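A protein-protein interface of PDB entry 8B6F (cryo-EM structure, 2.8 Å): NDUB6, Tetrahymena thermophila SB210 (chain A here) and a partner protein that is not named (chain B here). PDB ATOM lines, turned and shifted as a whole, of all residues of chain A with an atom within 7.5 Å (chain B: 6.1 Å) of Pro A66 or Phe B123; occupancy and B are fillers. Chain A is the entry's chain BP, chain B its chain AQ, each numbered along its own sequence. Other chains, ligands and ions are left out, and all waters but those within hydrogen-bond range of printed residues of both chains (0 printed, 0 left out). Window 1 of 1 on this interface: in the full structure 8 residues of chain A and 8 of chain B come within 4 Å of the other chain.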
ATOM      1  N   TYR A  63     -24.032  22.219  20.214  1.00  0.00           N
ATOM      2  CA  TYR A  63     -23.864  22.557  21.615  1.00  0.00           C
ATOM      3  C   TYR A  63     -22.722  21.744  22.207  1.00  0.00           C
ATOM      4  O   TYR A  63     -22.404  20.661  21.708  1.00  0.00           O
ATOM      5  CB  TYR A  63     -25.153  22.291  22.405  1.00  0.00           C
ATOM      6  CG  TYR A  63     -25.748  20.926  22.158  1.00  0.00           C
ATOM      7  CD1 TYR A  63     -25.346  19.828  22.904  1.00  0.00           C
ATOM      8  CD2 TYR A  63     -26.718  20.738  21.185  1.00  0.00           C
ATOM      9  CE1 TYR A  63     -25.888  18.578  22.683  1.00  0.00           C
ATOM     10  CE2 TYR A  63     -27.266  19.492  20.956  1.00  0.00           C
ATOM     11  CZ  TYR A  63     -26.847  18.417  21.708  1.00  0.00           C
ATOM     12  OH  TYR A  63     -27.389  17.174  21.486  1.00  0.00           O
ATOM     13  N   PRO A  64     -22.084  22.245  23.264  1.00  0.00           N
ATOM     14  CA  PRO A  64     -20.933  21.531  23.831  1.00  0.00           C
ATOM     15  C   PRO A  64     -21.313  20.162  24.376  1.00  0.00           C
ATOM     16  O   PRO A  64     -22.402  19.960  24.914  1.00  0.00           O
ATOM     17  CB  PRO A  64     -20.451  22.464  24.949  1.00  0.00           C
ATOM     18  CG  PRO A  64     -21.626  23.310  25.276  1.00  0.00           C
ATOM     19  CD  PRO A  64     -22.369  23.492  23.993  1.00  0.00           C
ATOM     20  N   ILE A  65     -20.384  19.221  24.237  1.00  0.00           N
ATOM     21  CA  ILE A  65     -20.536  17.861  24.735  1.00  0.00           C
ATOM     22  C   ILE A  65     -19.431  17.627  25.756  1.00  0.00           C
ATOM     23  O   ILE A  65     -18.275  17.953  25.481  1.00  0.00           O
ATOM     24  CB  ILE A  65     -20.452  16.811  23.612  1.00  0.00           C
ATOM     25  CG1 ILE A  65     -21.465  17.118  22.503  1.00  0.00           C
ATOM     26  CG2 ILE A  65     -20.665  15.409  24.168  1.00  0.00           C
ATOM     27  CD1 ILE A  65     -22.913  17.071  22.941  1.00  0.00           C
ATOM     28  N   PRO A  66     -19.726  17.075  26.934  1.00  0.00           N
ATOM     29  CA  PRO A  66     -18.663  16.878  27.927  1.00  0.00           C
ATOM     30  C   PRO A  66     -17.553  15.985  27.394  1.00  0.00           C
ATOM     31  O   PRO A  66     -17.800  14.999  26.699  1.00  0.00           O
ATOM     32  CB  PRO A  66     -19.396  16.225  29.106  1.00  0.00           C
ATOM     33  CG  PRO A  66     -20.637  15.656  28.525  1.00  0.00           C
ATOM     34  CD  PRO A  66     -21.022  16.579  27.418  1.00  0.00           C
ATOM     35  N   ARG A  67     -16.313  16.343  27.733  1.00  0.00           N
ATOM     36  CA  ARG A  67     -15.165  15.578  27.256  1.00  0.00           C
ATOM     37  C   ARG A  67     -15.144  14.176  27.852  1.00  0.00           C
ATOM     38  O   ARG A  67     -14.818  13.205  27.160  1.00  0.00           O
ATOM     39  CB  ARG A  67     -13.869  16.314  27.594  1.00  0.00           C
ATOM     40  CG  ARG A  67     -13.723  17.686  26.953  1.00  0.00           C
ATOM     41  CD  ARG A  67     -13.275  17.594  25.504  1.00  0.00           C
ATOM     42  NE  ARG A  67     -14.347  17.163  24.615  1.00  0.00           N
ATOM     43  CZ  ARG A  67     -15.217  17.977  24.034  1.00  0.00           C
ATOM     44  NH1 ARG A  67     -15.178  19.285  24.227  1.00  0.00           N
ATOM     45  NH2 ARG A  67     -16.152  17.466  23.241  1.00  0.00           N
ATOM     46  N   TYR A  68     -15.485  14.049  29.134  1.00  0.00           N
ATOM     47  CA  TYR A  68     -15.382  12.759  29.807  1.00  0.00           C
ATOM     48  C   TYR A  68     -16.361  11.733  29.258  1.00  0.00           C
ATOM     49  O   TYR A  68     -16.137  10.530  29.431  1.00  0.00           O
ATOM     50  CB  TYR A  68     -15.623  12.926  31.308  1.00  0.00           C
ATOM     51  CG  TYR A  68     -17.074  12.777  31.711  1.00  0.00           C
ATOM     52  CD1 TYR A  68     -17.952  13.849  31.630  1.00  0.00           C
ATOM     53  CD2 TYR A  68     -17.561  11.563  32.176  1.00  0.00           C
ATOM     54  CE1 TYR A  68     -19.276  13.714  31.998  1.00  0.00           C
ATOM     55  CE2 TYR A  68     -18.880  11.419  32.545  1.00  0.00           C
ATOM     56  CZ  TYR A  68     -19.732  12.496  32.454  1.00  0.00           C
ATOM     57  OH  TYR A  68     -21.047  12.349  32.824  1.00  0.00           O
ATOM     58  N   LEU A  69     -17.435  12.171  28.611  1.00  0.00           N
ATOM     59  CA  LEU A  69     -18.498  11.276  28.184  1.00  0.00           C
ATOM     60  C   LEU A  69     -18.194  10.727  26.796  1.00  0.00           C
ATOM     61  O   LEU A  69     -17.968  11.491  25.853  1.00  0.00           O
ATOM     62  CB  LEU A  69     -19.838  12.012  28.188  1.00  0.00           C
ATOM     63  CG  LEU A  69     -21.093  11.144  28.102  1.00  0.00           C
ATOM     64  CD1 LEU A  69     -21.211  10.209  29.295  1.00  0.00           C
ATOM     65  CD2 LEU A  69     -22.334  12.014  27.973  1.00  0.00           C
ATOM     66  N   HIS A  70     -18.193   9.399  26.678  1.00  0.00           N
ATOM     67  CA  HIS A  70     -17.884   8.722  25.419  1.00  0.00           C
ATOM     68  C   HIS A  70     -19.167   8.607  24.606  1.00  0.00           C
ATOM     69  O   HIS A  70     -19.862   7.593  24.641  1.00  0.00           O
ATOM     70  CB  HIS A  70     -17.266   7.359  25.694  1.00  0.00           C
ATOM     71  CG  HIS A  70     -16.668   6.710  24.487  1.00  0.00           C
ATOM     72  ND1 HIS A  70     -16.270   5.390  24.475  1.00  0.00           N
ATOM     73  CD2 HIS A  70     -16.404   7.194  23.253  1.00  0.00           C
ATOM     74  CE1 HIS A  70     -15.783   5.091  23.284  1.00  0.00           C
ATOM     75  NE2 HIS A  70     -15.854   6.169  22.524  1.00  0.00           N
ATOM     76  N   VAL A  71     -19.482   9.666  23.857  1.00  0.00           N
ATOM     77  CA  VAL A  71     -20.695   9.741  23.057  1.00  0.00           C
ATOM     78  C   VAL A  71     -20.337  10.156  21.637  1.00  0.00           C
ATOM     79  O   VAL A  71     -19.262  10.698  21.373  1.00  0.00           O
ATOM     80  CB  VAL A  71     -21.732  10.712  23.656  1.00  0.00           C
ATOM     81  CG1 VAL A  71     -22.381  10.087  24.868  1.00  0.00           C
ATOM     82  CG2 VAL A  71     -21.079  12.039  24.014  1.00  0.00           C
ATOM     83  N   GLN A  73     -21.930  12.365  19.586  1.00  0.00           N
ATOM     84  CA  GLN A  73     -22.438  13.639  19.089  1.00  0.00           C
ATOM     85  C   GLN A  73     -21.367  14.394  18.313  1.00  0.00           C
ATOM     86  O   GLN A  73     -20.384  14.861  18.895  1.00  0.00           O
ATOM     87  CB  GLN A  73     -22.950  14.506  20.243  1.00  0.00           C
ATOM     88  CG  GLN A  73     -24.312  14.102  20.789  1.00  0.00           C
ATOM     89  CD  GLN A  73     -24.293  12.756  21.475  1.00  0.00           C
ATOM     90  OE1 GLN A  73     -23.512  11.875  21.118  1.00  0.00           O
ATOM     91  NE2 GLN A  73     -25.152  12.587  22.472  1.00  0.00           N
ATOM     92  N   TYR B 121     -30.630  16.491  24.235  1.00  0.00           N
ATOM     93  CA  TYR B 121     -30.361  16.689  25.653  1.00  0.00           C
ATOM     94  C   TYR B 121     -29.151  17.603  25.793  1.00  0.00           C
ATOM     95  O   TYR B 121     -28.047  17.248  25.365  1.00  0.00           O
ATOM     96  CB  TYR B 121     -30.112  15.351  26.349  1.00  0.00           C
ATOM     97  CG  TYR B 121     -29.639  15.476  27.779  1.00  0.00           C
ATOM     98  CD1 TYR B 121     -30.486  15.941  28.776  1.00  0.00           C
ATOM     99  CD2 TYR B 121     -28.350  15.110  28.132  1.00  0.00           C
ATOM    100  CE1 TYR B 121     -30.055  16.050  30.083  1.00  0.00           C
ATOM    101  CE2 TYR B 121     -27.911  15.214  29.435  1.00  0.00           C
ATOM    102  CZ  TYR B 121     -28.768  15.683  30.405  1.00  0.00           C
ATOM    103  OH  TYR B 121     -28.331  15.787  31.704  1.00  0.00           O
ATOM    104  N   ILE B 122     -29.359  18.769  26.392  1.00  0.00           N
ATOM    105  CA  ILE B 122     -28.314  19.776  26.526  1.00  0.00           C
ATOM    106  C   ILE B 122     -27.546  19.519  27.813  1.00  0.00           C
ATOM    107  O   ILE B 122     -28.140  19.411  28.892  1.00  0.00           O
ATOM    108  CB  ILE B 122     -28.916  21.190  26.514  1.00  0.00           C
ATOM    109  CG1 ILE B 122     -29.883  21.355  25.338  1.00  0.00           C
ATOM    110  CG2 ILE B 122     -27.818  22.236  26.444  1.00  0.00           C
ATOM    111  CD1 ILE B 122     -29.282  21.045  23.986  1.00  0.00           C
ATOM    112  N   PHE B 123     -26.224  19.421  27.703  1.00  0.00           N
ATOM    113  CA  PHE B 123     -25.390  19.106  28.853  1.00  0.00           C
ATOM    114  C   PHE B 123     -25.068  20.366  29.645  1.00  0.00           C
ATOM    115  O   PHE B 123     -24.713  21.403  29.077  1.00  0.00           O
ATOM    116  CB  PHE B 123     -24.102  18.422  28.401  1.00  0.00           C
ATOM    117  CG  PHE B 123     -24.328  17.101  27.728  1.00  0.00           C
ATOM    118  CD1 PHE B 123     -24.434  15.940  28.473  1.00  0.00           C
ATOM    119  CD2 PHE B 123     -24.434  17.020  26.351  1.00  0.00           C
ATOM    120  CE1 PHE B 123     -24.641  14.722  27.859  1.00  0.00           C
ATOM    121  CE2 PHE B 123     -24.643  15.805  25.730  1.00  0.00           C
ATOM    122  CZ  PHE B 123     -24.746  14.654  26.485  1.00  0.00           C
ATOM    123  N   ASP B 124     -25.188  20.264  30.965  1.00  0.00           N
ATOM    124  CA  ASP B 124     -24.989  21.395  31.858  1.00  0.00           C
ATOM    125  C   ASP B 124     -23.506  21.591  32.158  1.00  0.00           C
ATOM    126  O   ASP B 124     -22.679  20.698  31.955  1.00  0.00           O
ATOM    127  CB  ASP B 124     -25.760  21.184  33.160  1.00  0.00           C
ATOM    128  CG  ASP B 124     -25.792  22.426  34.026  1.00  0.00           C
ATOM    129  OD1 ASP B 124     -26.538  23.369  33.689  1.00  0.00           O
ATOM    130  OD2 ASP B 124     -25.072  22.461  35.045  1.00  0.00           O
ATOM    131  N   ASP B 125     -23.175  22.783  32.662  1.00  0.00           N
ATOM    132  CA  ASP B 125     -21.788  23.080  33.005  1.00  0.00           C
ATOM    133  C   ASP B 125     -21.243  22.105  34.039  1.00  0.00           C
ATOM    134  O   ASP B 125     -20.032  21.868  34.087  1.00  0.00           O
ATOM    135  CB  ASP B 125     -21.662  24.514  33.519  1.00  0.00           C
ATOM    136  CG  ASP B 125     -21.565  25.528  32.399  1.00  0.00           C
ATOM    137  OD1 ASP B 125     -21.070  25.170  31.312  1.00  0.00           O
ATOM    138  OD2 ASP B 125     -21.977  26.689  32.606  1.00  0.00           O
ATOM    139  N   LEU B 127     -21.795  18.804  34.105  1.00  0.00           N
ATOM    140  CA  LEU B 127     -21.275  17.688  33.321  1.00  0.00           C
ATOM    141  C   LEU B 127     -20.049  18.101  32.518  1.00  0.00           C
ATOM    142  O   LEU B 127     -19.098  17.323  32.385  1.00  0.00           O
ATOM    143  CB  LEU B 127     -22.365  17.146  32.398  1.00  0.00           C
ATOM    144  CG  LEU B 127     -23.540  16.467  33.103  1.00  0.00           C
ATOM    145  CD1 LEU B 127     -24.631  16.126  32.111  1.00  0.00           C
ATOM    146  CD2 LEU B 127     -23.083  15.217  33.837  1.00  0.00           C
ATOM    147  N   LEU B 128     -20.055  19.316  31.967  1.00  0.00           N
ATOM    148  CA  LEU B 128     -18.916  19.772  31.180  1.00  0.00           C
ATOM    149  C   LEU B 128     -17.652  19.842  32.027  1.00  0.00           C
ATOM    150  O   LEU B 128     -16.573  19.439  31.580  1.00  0.00           O
ATOM    151  CB  LEU B 128     -19.222  21.132  30.552  1.00  0.00           C
ATOM    152  CG  LEU B 128     -20.423  21.184  29.600  1.00  0.00           C
ATOM    153  CD1 LEU B 128     -20.608  22.584  29.047  1.00  0.00           C
ATOM    154  CD2 LEU B 128     -20.283  20.183  28.467  1.00  0.00           C
ATOM    155  N   LYS B 129     -17.767  20.349  33.256  1.00  0.00           N
ATOM    156  CA  LYS B 129     -16.605  20.421  34.138  1.00  0.00           C
ATOM    157  C   LYS B 129     -16.191  19.041  34.630  1.00  0.00           C
ATOM    158  O   LYS B 129     -14.998  18.773  34.809  1.00  0.00           O
ATOM    159  CB  LYS B 129     -16.901  21.329  35.331  1.00  0.00           C
ATOM    160  CG  LYS B 129     -17.048  22.799  34.980  1.00  0.00           C
ATOM    161  CD  LYS B 129     -17.086  23.674  36.227  1.00  0.00           C
ATOM    162  CE  LYS B 129     -18.182  23.252  37.196  1.00  0.00           C
ATOM    163  NZ  LYS B 129     -19.516  23.175  36.542  1.00  0.00           N
ATOM    164  N   PHE B 130     -17.159  18.159  34.863  1.00  0.00           N
ATOM    165  CA  PHE B 130     -16.877  16.865  35.471  1.00  0.00           C
ATOM    166  C   PHE B 130     -15.789  16.129  34.706  1.00  0.00           C
ATOM    167  O   PHE B 130     -15.915  15.877  33.505  1.00  0.00           O
ATOM    168  CB  PHE B 130     -18.156  16.029  35.519  1.00  0.00           C
ATOM    169  CG  PHE B 130     -17.992  14.724  36.233  1.00  0.00           C
ATOM    170  CD1 PHE B 130     -17.803  14.691  37.603  1.00  0.00           C
ATOM    171  CD2 PHE B 130     -18.038  13.530  35.539  1.00  0.00           C
ATOM    172  CE1 PHE B 130     -17.654  13.490  38.266  1.00  0.00           C
ATOM    173  CE2 PHE B 130     -17.891  12.328  36.196  1.00  0.00           C
ATOM    174  CZ  PHE B 130     -17.699  12.307  37.561  1.00  0.00           C
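The guanidinium group (NH2) of Arg A67 lies within hydrogen-bond range of the backbone carbonyl oxygen (O) of Ile A65.
Among the printed residues, merely in contact across the chains: Tyr A63 with Tyr B121 (3.7 Å), Tyr A63 with Ile B122 (3.8 Å), Pro A64 with Phe B123 (3.9 Å), Pro A64 with Leu B128 (3.97 Å), Ile A65 with Phe B123 (3.5 Å), Ile A65 with Leu B128 (3.8 Å), Pro A66 with Phe B123 (3.4 Å), Pro A66 with Leu B127 (3.5 Å), Pro A66 with Leu B128 (3.5 Å), Tyr A68 with Leu B127 (3.6 Å), Tyr A68 with Phe B130 (3.4 Å) and Leu A69 with Phe B123 (3.6 Å).
Pro A66 touches just these residues of chain B: Phe B123, Leu B127 and Leu B128.
Phe B123 touches just these residues of chain A: Pro A64, Ile A65, Pro A66 and Leu A69.
Of the printed residues of chain B, Tyr A63 touches Tyr B121 and Ile B122.
Of the printed residues of chain B, Pro A64 touches Phe B123 and Leu B128.
Printed residues of chain A within 4 Å of Leu B128: Pro A64, Ile A65 and Pro A66.
Of the printed residues of chain A, Leu B127 touches Pro A66 and Tyr A68.
The nearest residue of chain B that does not touch Pro A66 is Phe B130 (5.6 Å).
Along chain B the printed residues that touch a printed residue of chain A span positions 121 to 130.
Of the 10 printed residues of chain A, 6 touch a printed residue of chain B.
Hydrophobic or aromatic side chains of chain A within 4 Å of the printed part of chain B: Tyr A63, Pro A64, Ile A65, Pro A66, Tyr A68 and Leu A69.
Along chain A the printed residues that touch a printed residue of chain B span positions 63 to 69.
Among the printed residues, no Asp or Glu carboxylate lies within 4 Å of a Lys or Arg side-chain nitrogen of the other chain.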
